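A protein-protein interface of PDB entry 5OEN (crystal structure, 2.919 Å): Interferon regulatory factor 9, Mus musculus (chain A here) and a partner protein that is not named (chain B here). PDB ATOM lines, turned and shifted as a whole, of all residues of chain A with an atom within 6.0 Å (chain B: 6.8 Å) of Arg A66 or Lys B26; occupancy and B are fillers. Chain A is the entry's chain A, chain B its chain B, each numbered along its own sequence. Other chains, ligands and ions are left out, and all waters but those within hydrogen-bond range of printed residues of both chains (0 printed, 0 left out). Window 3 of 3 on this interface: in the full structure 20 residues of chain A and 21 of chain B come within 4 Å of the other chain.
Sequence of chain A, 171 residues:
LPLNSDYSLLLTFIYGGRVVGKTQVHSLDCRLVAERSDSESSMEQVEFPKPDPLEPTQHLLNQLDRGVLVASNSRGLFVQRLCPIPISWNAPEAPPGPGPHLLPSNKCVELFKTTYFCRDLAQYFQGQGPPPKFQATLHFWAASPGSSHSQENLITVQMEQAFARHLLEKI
The side-chain carboxylate (OD2) of Asp B27 is in salt-bridge range of the guanidinium group (NH2) of Arg A31. OD1 of Asp A65 lies within salt-bridge range of NH2 of Arg B23 (3.5 Å). NE of Arg A66 is in salt-bridge range of OD2 of Asp B30, 3.96 Å away.
The side-chain amino group of Lys B26 lies within salt-bridge range of the side-chain carboxylate of Asp B30, 3.1 Å away.
Among the printed residues, merely in contact across the chains: Arg A66 with Lys B26 (3.8 Å).
Of the printed residues of chain A, Lys B26 touches Arg A66 (3.8 Å). Printed residues of chain B within 4 Å of Arg A31: Asp B27. Printed residues of chain A within 4 Å of Arg B23: Asp A65. The nearest printed residue of chain A that does not touch Lys B26 is Arg A31 (6.5 Å). The nearest printed residue of chain A that does not touch Arg B23 is Arg A66 (5.9 Å).
Printed residues of chain A that touch a printed residue of chain B: Arg A31, Asp A65 and Arg A66. Of the 13 printed residues of chain B, 4 touch a printed residue of chain A. Printed residues of chain B that touch a printed residue of chain A: Arg B23, Lys B26, Asp B27 and Asp B30. Among the printed residues, 4 pairs touch across the chains.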
ATOM      1  N   ARG A  31     -22.744 -27.320  -4.246  1.00  0.00           N
ATOM      2  CA  ARG A  31     -23.365 -26.003  -4.245  1.00  0.00           C
ATOM      3  C   ARG A  31     -23.835 -25.694  -2.833  1.00  0.00           C
ATOM      4  O   ARG A  31     -24.556 -26.490  -2.225  1.00  0.00           O
ATOM      5  CB  ARG A  31     -24.535 -25.927  -5.230  1.00  0.00           C
ATOM      6  CG  ARG A  31     -25.176 -24.547  -5.308  1.00  0.00           C
ATOM      7  CD  ARG A  31     -25.778 -24.270  -6.675  1.00  0.00           C
ATOM      8  NE  ARG A  31     -27.055 -24.941  -6.890  1.00  0.00           N
ATOM      9  CZ  ARG A  31     -27.647 -25.042  -8.077  1.00  0.00           C
ATOM     10  NH1 ARG A  31     -27.079 -24.519  -9.158  1.00  0.00           N
ATOM     11  NH2 ARG A  31     -28.809 -25.671  -8.187  1.00  0.00           N
ATOM     12  N   LEU A  32     -23.419 -24.543  -2.318  1.00  0.00           N
ATOM     13  CA  LEU A  32     -23.791 -24.113  -0.979  1.00  0.00           C
ATOM     14  C   LEU A  32     -25.067 -23.287  -1.059  1.00  0.00           C
ATOM     15  O   LEU A  32     -25.077 -22.205  -1.658  1.00  0.00           O
ATOM     16  CB  LEU A  32     -22.658 -23.306  -0.346  1.00  0.00           C
ATOM     17  CG  LEU A  32     -21.272 -23.942  -0.494  1.00  0.00           C
ATOM     18  CD1 LEU A  32     -20.200 -23.087   0.159  1.00  0.00           C
ATOM     19  CD2 LEU A  32     -21.245 -25.356   0.078  1.00  0.00           C
ATOM     20  N   VAL A  33     -26.139 -23.794  -0.450  1.00  0.00           N
ATOM     21  CA  VAL A  33     -27.460 -23.193  -0.558  1.00  0.00           C
ATOM     22  C   VAL A  33     -28.059 -23.051   0.834  1.00  0.00           C
ATOM     23  O   VAL A  33     -27.654 -23.721   1.784  1.00  0.00           O
ATOM     24  CB  VAL A  33     -28.403 -24.021  -1.459  1.00  0.00           C
ATOM     25  CG1 VAL A  33     -27.828 -24.133  -2.852  1.00  0.00           C
ATOM     26  CG2 VAL A  33     -28.634 -25.410  -0.874  1.00  0.00           C
ATOM     27  N   GLN A  63     -31.360 -14.713   0.821  1.00  0.00           N
ATOM     28  CA  GLN A  63     -31.061 -14.000  -0.413  1.00  0.00           C
ATOM     29  C   GLN A  63     -30.041 -14.727  -1.278  1.00  0.00           C
ATOM     30  O   GLN A  63     -29.729 -14.250  -2.375  1.00  0.00           O
ATOM     31  CB  GLN A  63     -30.551 -12.588  -0.101  1.00  0.00           C
ATOM     32  CG  GLN A  63     -31.523 -11.732   0.689  1.00  0.00           C
ATOM     33  CD  GLN A  63     -30.903 -10.425   1.134  1.00  0.00           C
ATOM     34  OE1 GLN A  63     -30.370  -9.670   0.321  1.00  0.00           O
ATOM     35  NE2 GLN A  63     -30.958 -10.155   2.433  1.00  0.00           N
ATOM     36  N   LEU A  64     -29.511 -15.862  -0.817  1.00  0.00           N
ATOM     37  CA  LEU A  64     -28.575 -16.626  -1.635  1.00  0.00           C
ATOM     38  C   LEU A  64     -29.209 -17.021  -2.961  1.00  0.00           C
ATOM     39  O   LEU A  64     -28.654 -16.758  -4.035  1.00  0.00           O
ATOM     40  CB  LEU A  64     -28.111 -17.871  -0.880  1.00  0.00           C
ATOM     41  CG  LEU A  64     -27.120 -17.685   0.268  1.00  0.00           C
ATOM     42  CD1 LEU A  64     -26.899 -19.016   0.969  1.00  0.00           C
ATOM     43  CD2 LEU A  64     -25.796 -17.124  -0.229  1.00  0.00           C
ATOM     44  N   ASP A  65     -30.370 -17.668  -2.905  1.00  0.00           N
ATOM     45  CA  ASP A  65     -31.043 -18.150  -4.103  1.00  0.00           C
ATOM     46  C   ASP A  65     -30.173 -19.188  -4.809  1.00  0.00           C
ATOM     47  O   ASP A  65     -30.086 -20.334  -4.360  1.00  0.00           O
ATOM     48  CB  ASP A  65     -31.393 -16.978  -5.028  1.00  0.00           C
ATOM     49  CG  ASP A  65     -32.210 -17.408  -6.233  1.00  0.00           C
ATOM     50  OD1 ASP A  65     -33.362 -17.854  -6.042  1.00  0.00           O
ATOM     51  OD2 ASP A  65     -31.700 -17.303  -7.369  1.00  0.00           O
ATOM     52  N   ARG A  66     -29.517 -18.805  -5.907  1.00  0.00           N
ATOM     53  CA  ARG A  66     -28.704 -19.762  -6.650  1.00  0.00           C
ATOM     54  C   ARG A  66     -27.528 -20.270  -5.820  1.00  0.00           C
ATOM     55  O   ARG A  66     -27.100 -21.418  -5.988  1.00  0.00           O
ATOM     56  CB  ARG A  66     -28.218 -19.122  -7.952  1.00  0.00           C
ATOM     57  CG  ARG A  66     -29.328 -18.934  -8.983  1.00  0.00           C
ATOM     58  CD  ARG A  66     -29.140 -17.671  -9.811  1.00  0.00           C
ATOM     59  NE  ARG A  66     -28.068 -17.789 -10.796  1.00  0.00           N
ATOM     60  CZ  ARG A  66     -27.643 -16.787 -11.561  1.00  0.00           C
ATOM     61  NH1 ARG A  66     -28.192 -15.584 -11.453  1.00  0.00           N
ATOM     62  NH2 ARG A  66     -26.664 -16.984 -12.433  1.00  0.00           N
ATOM     63  N   GLY A  67     -26.991 -19.439  -4.930  1.00  0.00           N
ATOM     64  CA  GLY A  67     -25.962 -19.882  -4.008  1.00  0.00           C
ATOM     65  C   GLY A  67     -24.556 -19.747  -4.551  1.00  0.00           C
ATOM     66  O   GLY A  67     -24.286 -18.892  -5.399  1.00  0.00           O
ATOM     67  N   VAL A  68     -23.651 -20.596  -4.067  1.00  0.00           N
ATOM     68  CA  VAL A  68     -22.242 -20.567  -4.444  1.00  0.00           C
ATOM     69  C   VAL A  68     -21.842 -21.945  -4.949  1.00  0.00           C
ATOM     70  O   VAL A  68     -22.232 -22.967  -4.375  1.00  0.00           O
ATOM     71  CB  VAL A  68     -21.344 -20.147  -3.262  1.00  0.00           C
ATOM     72  CG1 VAL A  68     -19.893 -20.013  -3.710  1.00  0.00           C
ATOM     73  CG2 VAL A  68     -21.837 -18.847  -2.650  1.00  0.00           C
ATOM     74  N   LEU A  69     -21.052 -21.964  -6.019  1.00  0.00           N
ATOM     75  CA  LEU A  69     -20.504 -23.189  -6.587  1.00  0.00           C
ATOM     76  C   LEU A  69     -19.036 -23.309  -6.205  1.00  0.00           C
ATOM     77  O   LEU A  69     -18.262 -22.367  -6.401  1.00  0.00           O
ATOM     78  CB  LEU A  69     -20.636 -23.192  -8.112  1.00  0.00           C
ATOM     79  CG  LEU A  69     -22.047 -23.187  -8.693  1.00  0.00           C
ATOM     80  CD1 LEU A  69     -21.982 -23.026 -10.196  1.00  0.00           C
ATOM     81  CD2 LEU A  69     -22.752 -24.470  -8.347  1.00  0.00           C
ATOM     82  N   ARG A  81     -19.681 -17.320  -7.926  1.00  0.00           N
ATOM     83  CA  ARG A  81     -20.764 -16.716  -7.162  1.00  0.00           C
ATOM     84  C   ARG A  81     -21.973 -16.489  -8.060  1.00  0.00           C
ATOM     85  O   ARG A  81     -21.866 -15.838  -9.104  1.00  0.00           O
ATOM     86  CB  ARG A  81     -20.308 -15.393  -6.547  1.00  0.00           C
ATOM     87  CG  ARG A  81     -21.385 -14.676  -5.750  1.00  0.00           C
ATOM     88  CD  ARG A  81     -20.845 -13.407  -5.116  1.00  0.00           C
ATOM     89  NE  ARG A  81     -20.624 -12.349  -6.099  1.00  0.00           N
ATOM     90  CZ  ARG A  81     -21.502 -11.399  -6.407  1.00  0.00           C
ATOM     91  NH1 ARG A  81     -22.686 -11.351  -5.810  1.00  0.00           N
ATOM     92  NH2 ARG A  81     -21.194 -10.484  -7.317  1.00  0.00           N
ATOM     93  N   LEU A  82     -23.121 -17.023  -7.648  1.00  0.00           N
ATOM     94  CA  LEU A  82     -24.365 -16.877  -8.392  1.00  0.00           C
ATOM     95  C   LEU A  82     -25.410 -16.059  -7.646  1.00  0.00           C
ATOM     96  O   LEU A  82     -26.501 -15.836  -8.183  1.00  0.00           O
ATOM     97  CB  LEU A  82     -24.945 -18.256  -8.723  1.00  0.00           C
ATOM     98  CG  LEU A  82     -24.038 -19.200  -9.511  1.00  0.00           C
ATOM     99  CD1 LEU A  82     -24.709 -20.551  -9.680  1.00  0.00           C
ATOM    100  CD2 LEU A  82     -23.680 -18.602 -10.864  1.00  0.00           C
ATOM    101  N   CYS A  83     -25.107 -15.605  -6.437  1.00  0.00           N
ATOM    102  CA  CYS A  83     -26.057 -14.896  -5.599  1.00  0.00           C
ATOM    103  C   CYS A  83     -25.815 -13.397  -5.659  1.00  0.00           C
ATOM    104  O   CYS A  83     -24.719 -12.942  -5.999  1.00  0.00           O
ATOM    105  CB  CYS A  83     -25.941 -15.380  -4.150  1.00  0.00           C
ATOM    106  SG  CYS A  83     -24.273 -15.267  -3.460  1.00  0.00           S
ATOM    107  N   SER A 105     -19.676 -11.838 -10.414  1.00  0.00           N
ATOM    108  CA  SER A 105     -20.767 -12.660 -10.918  1.00  0.00           C
ATOM    109  C   SER A 105     -20.476 -13.097 -12.348  1.00  0.00           C
ATOM    110  O   SER A 105     -19.939 -12.331 -13.154  1.00  0.00           O
ATOM    111  CB  SER A 105     -22.084 -11.887 -10.860  1.00  0.00           C
ATOM    112  OG  SER A 105     -23.148 -12.642 -11.414  1.00  0.00           O
ATOM    113  N   SER B  21     -39.886 -26.940 -13.896  1.00  0.00           N
ATOM    114  CA  SER B  21     -38.987 -27.642 -14.807  1.00  0.00           C
ATOM    115  C   SER B  21     -38.001 -26.679 -15.455  1.00  0.00           C
ATOM    116  O   SER B  21     -36.818 -27.004 -15.619  1.00  0.00           O
ATOM    117  CB  SER B  21     -39.795 -28.375 -15.879  1.00  0.00           C
ATOM    118  OG  SER B  21     -40.570 -29.423 -15.320  1.00  0.00           O
ATOM    119  N   ILE B  22     -38.470 -25.489 -15.832  1.00  0.00           N
ATOM    120  CA  ILE B  22     -37.597 -24.514 -16.477  1.00  0.00           C
ATOM    121  C   ILE B  22     -36.543 -24.014 -15.497  1.00  0.00           C
ATOM    122  O   ILE B  22     -35.390 -23.775 -15.874  1.00  0.00           O
ATOM    123  CB  ILE B  22     -38.432 -23.357 -17.054  1.00  0.00           C
ATOM    124  CG1 ILE B  22     -39.400 -23.888 -18.117  1.00  0.00           C
ATOM    125  CG2 ILE B  22     -37.527 -22.297 -17.663  1.00  0.00           C
ATOM    126  CD1 ILE B  22     -40.495 -22.920 -18.484  1.00  0.00           C
ATOM    127  N   ARG B  23     -36.920 -23.839 -14.227  1.00  0.00           N
ATOM    128  CA  ARG B  23     -35.938 -23.465 -13.214  1.00  0.00           C
ATOM    129  C   ARG B  23     -34.919 -24.577 -13.012  1.00  0.00           C
ATOM    130  O   ARG B  23     -33.720 -24.311 -12.868  1.00  0.00           O
ATOM    131  CB  ARG B  23     -36.640 -23.136 -11.896  1.00  0.00           C
ATOM    132  CG  ARG B  23     -35.694 -22.731 -10.775  1.00  0.00           C
ATOM    133  CD  ARG B  23     -36.452 -22.301  -9.530  1.00  0.00           C
ATOM    134  NE  ARG B  23     -35.557 -21.807  -8.487  1.00  0.00           N
ATOM    135  CZ  ARG B  23     -35.963 -21.287  -7.333  1.00  0.00           C
ATOM    136  NH1 ARG B  23     -37.259 -21.185  -7.059  1.00  0.00           N
ATOM    137  NH2 ARG B  23     -35.070 -20.864  -6.449  1.00  0.00           N
ATOM    138  N   GLN B  24     -35.380 -25.829 -12.997  1.00  0.00           N
ATOM    139  CA  GLN B  24     -34.465 -26.960 -12.907  1.00  0.00           C
ATOM    140  C   GLN B  24     -33.464 -26.945 -14.056  1.00  0.00           C
ATOM    141  O   GLN B  24     -32.267 -27.176 -13.851  1.00  0.00           O
ATOM    142  CB  GLN B  24     -35.260 -28.266 -12.900  1.00  0.00           C
ATOM    143  CG  GLN B  24     -34.421 -29.516 -12.709  1.00  0.00           C
ATOM    144  CD  GLN B  24     -35.211 -30.784 -12.965  1.00  0.00           C
ATOM    145  OE1 GLN B  24     -35.154 -31.353 -14.056  1.00  0.00           O
ATOM    146  NE2 GLN B  24     -35.954 -31.233 -11.960  1.00  0.00           N
ATOM    147  N   LEU B  25     -33.939 -26.678 -15.275  1.00  0.00           N
ATOM    148  CA  LEU B  25     -33.043 -26.612 -16.424  1.00  0.00           C
ATOM    149  C   LEU B  25     -32.052 -25.466 -16.272  1.00  0.00           C
ATOM    150  O   LEU B  25     -30.839 -25.655 -16.413  1.00  0.00           O
ATOM    151  CB  LEU B  25     -33.852 -26.450 -17.711  1.00  0.00           C
ATOM    152  CG  LEU B  25     -33.042 -26.360 -19.007  1.00  0.00           C
ATOM    153  CD1 LEU B  25     -32.370 -27.687 -19.315  1.00  0.00           C
ATOM    154  CD2 LEU B  25     -33.926 -25.927 -20.163  1.00  0.00           C
ATOM    155  N   LYS B  26     -32.558 -24.264 -15.987  1.00  0.00           N
ATOM    156  CA  LYS B  26     -31.688 -23.108 -15.811  1.00  0.00           C
ATOM    157  C   LYS B  26     -30.586 -23.409 -14.802  1.00  0.00           C
ATOM    158  O   LYS B  26     -29.402 -23.165 -15.063  1.00  0.00           O
ATOM    159  CB  LYS B  26     -32.521 -21.902 -15.367  1.00  0.00           C
ATOM    160  CG  LYS B  26     -31.994 -20.555 -15.846  1.00  0.00           C
ATOM    161  CD  LYS B  26     -30.649 -20.215 -15.223  1.00  0.00           C
ATOM    162  CE  LYS B  26     -30.159 -18.850 -15.668  1.00  0.00           C
ATOM    163  NZ  LYS B  26     -28.769 -18.584 -15.204  1.00  0.00           N
ATOM    164  N   ASP B  27     -30.960 -23.955 -13.641  1.00  0.00           N
ATOM    165  CA  ASP B  27     -29.970 -24.295 -12.623  1.00  0.00           C
ATOM    166  C   ASP B  27     -28.888 -25.211 -13.181  1.00  0.00           C
ATOM    167  O   ASP B  27     -27.704 -25.053 -12.862  1.00  0.00           O
ATOM    168  CB  ASP B  27     -30.656 -24.955 -11.426  1.00  0.00           C
ATOM    169  CG  ASP B  27     -31.346 -23.952 -10.520  1.00  0.00           C
ATOM    170  OD1 ASP B  27     -31.430 -22.764 -10.899  1.00  0.00           O
ATOM    171  OD2 ASP B  27     -31.799 -24.351  -9.425  1.00  0.00           O
ATOM    172  N   GLU B  28     -29.276 -26.177 -14.015  1.00  0.00           N
ATOM    173  CA  GLU B  28     -28.314 -27.144 -14.532  1.00  0.00           C
ATOM    174  C   GLU B  28     -27.435 -26.560 -15.630  1.00  0.00           C
ATOM    175  O   GLU B  28     -26.266 -26.943 -15.745  1.00  0.00           O
ATOM    176  CB  GLU B  28     -29.044 -28.383 -15.049  1.00  0.00           C
ATOM    177  CG  GLU B  28     -29.163 -29.491 -14.017  1.00  0.00           C
ATOM    178  CD  GLU B  28     -27.967 -30.423 -14.017  1.00  0.00           C
ATOM    179  OE1 GLU B  28     -27.479 -30.763 -15.115  1.00  0.00           O
ATOM    180  OE2 GLU B  28     -27.511 -30.811 -12.921  1.00  0.00           O
ATOM    181  N   GLN B  29     -27.965 -25.646 -16.445  1.00  0.00           N
ATOM    182  CA  GLN B  29     -27.131 -25.016 -17.463  1.00  0.00           C
ATOM    183  C   GLN B  29     -25.996 -24.224 -16.832  1.00  0.00           C
ATOM    184  O   GLN B  29     -24.907 -24.131 -17.412  1.00  0.00           O
ATOM    185  CB  GLN B  29     -27.980 -24.122 -18.368  1.00  0.00           C
ATOM    186  CG  GLN B  29     -28.953 -24.896 -19.250  1.00  0.00           C
ATOM    187  CD  GLN B  29     -29.529 -24.058 -20.375  1.00  0.00           C
ATOM    188  OE1 GLN B  29     -29.190 -22.885 -20.531  1.00  0.00           O
ATOM    189  NE2 GLN B  29     -30.403 -24.662 -21.171  1.00  0.00           N
ATOM    190  N   ASP B  30     -26.223 -23.652 -15.646  1.00  0.00           N
ATOM    191  CA  ASP B  30     -25.131 -23.032 -14.902  1.00  0.00           C
ATOM    192  C   ASP B  30     -24.103 -24.072 -14.475  1.00  0.00           C
ATOM    193  O   ASP B  30     -22.893 -23.837 -14.575  1.00  0.00           O
ATOM    194  CB  ASP B  30     -25.676 -22.295 -13.677  1.00  0.00           C
ATOM    195  CG  ASP B  30     -26.602 -21.147 -14.042  1.00  0.00           C
ATOM    196  OD1 ASP B  30     -26.416 -20.540 -15.117  1.00  0.00           O
ATOM    197  OD2 ASP B  30     -27.517 -20.849 -13.243  1.00  0.00           O
ATOM    198  N   VAL B  31     -24.569 -25.228 -13.993  1.00  0.00           N
ATOM    199  CA  VAL B  31     -23.666 -26.305 -13.587  1.00  0.00           C
ATOM    200  C   VAL B  31     -22.721 -26.660 -14.729  1.00  0.00           C
ATOM    201  O   VAL B  31     -21.496 -26.701 -14.560  1.00  0.00           O
ATOM    202  CB  VAL B  31     -24.475 -27.529 -13.120  1.00  0.00           C
ATOM    203  CG1 VAL B  31     -23.567 -28.727 -12.865  1.00  0.00           C
ATOM    204  CG2 VAL B  31     -25.274 -27.187 -11.867  1.00  0.00           C
ATOM    205  N   MET B  68     -33.077 -32.793 -20.390  1.00  0.00           N
ATOM    206  CA  MET B  68     -34.040 -31.836 -19.856  1.00  0.00           C
ATOM    207  C   MET B  68     -34.597 -30.946 -20.960  1.00  0.00           C
ATOM    208  O   MET B  68     -35.813 -30.738 -21.047  1.00  0.00           O
ATOM    209  CB  MET B  68     -33.385 -30.989 -18.766  1.00  0.00           C
ATOM    210  CG  MET B  68     -33.027 -31.760 -17.510  1.00  0.00           C
ATOM    211  SD  MET B  68     -32.216 -30.731 -16.274  1.00  0.00           S
ATOM    212  CE  MET B  68     -32.036 -31.903 -14.932  1.00  0.00           C
ATOM    213  N   MET B 142     -32.022 -19.082 -22.782  1.00  0.00           N
ATOM    214  CA  MET B 142     -31.186 -20.218 -22.411  1.00  0.00           C
ATOM    215  C   MET B 142     -30.617 -20.912 -23.640  1.00  0.00           C
ATOM    216  O   MET B 142     -29.509 -21.456 -23.589  1.00  0.00           O
ATOM    217  CB  MET B 142     -31.993 -21.209 -21.573  1.00  0.00           C
ATOM    218  CG  MET B 142     -32.109 -20.829 -20.107  1.00  0.00           C
ATOM    219  SD  MET B 142     -33.361 -21.779 -19.228  1.00  0.00           S
ATOM    220  CE  MET B 142     -34.746 -20.653 -19.321  1.00  0.00           C
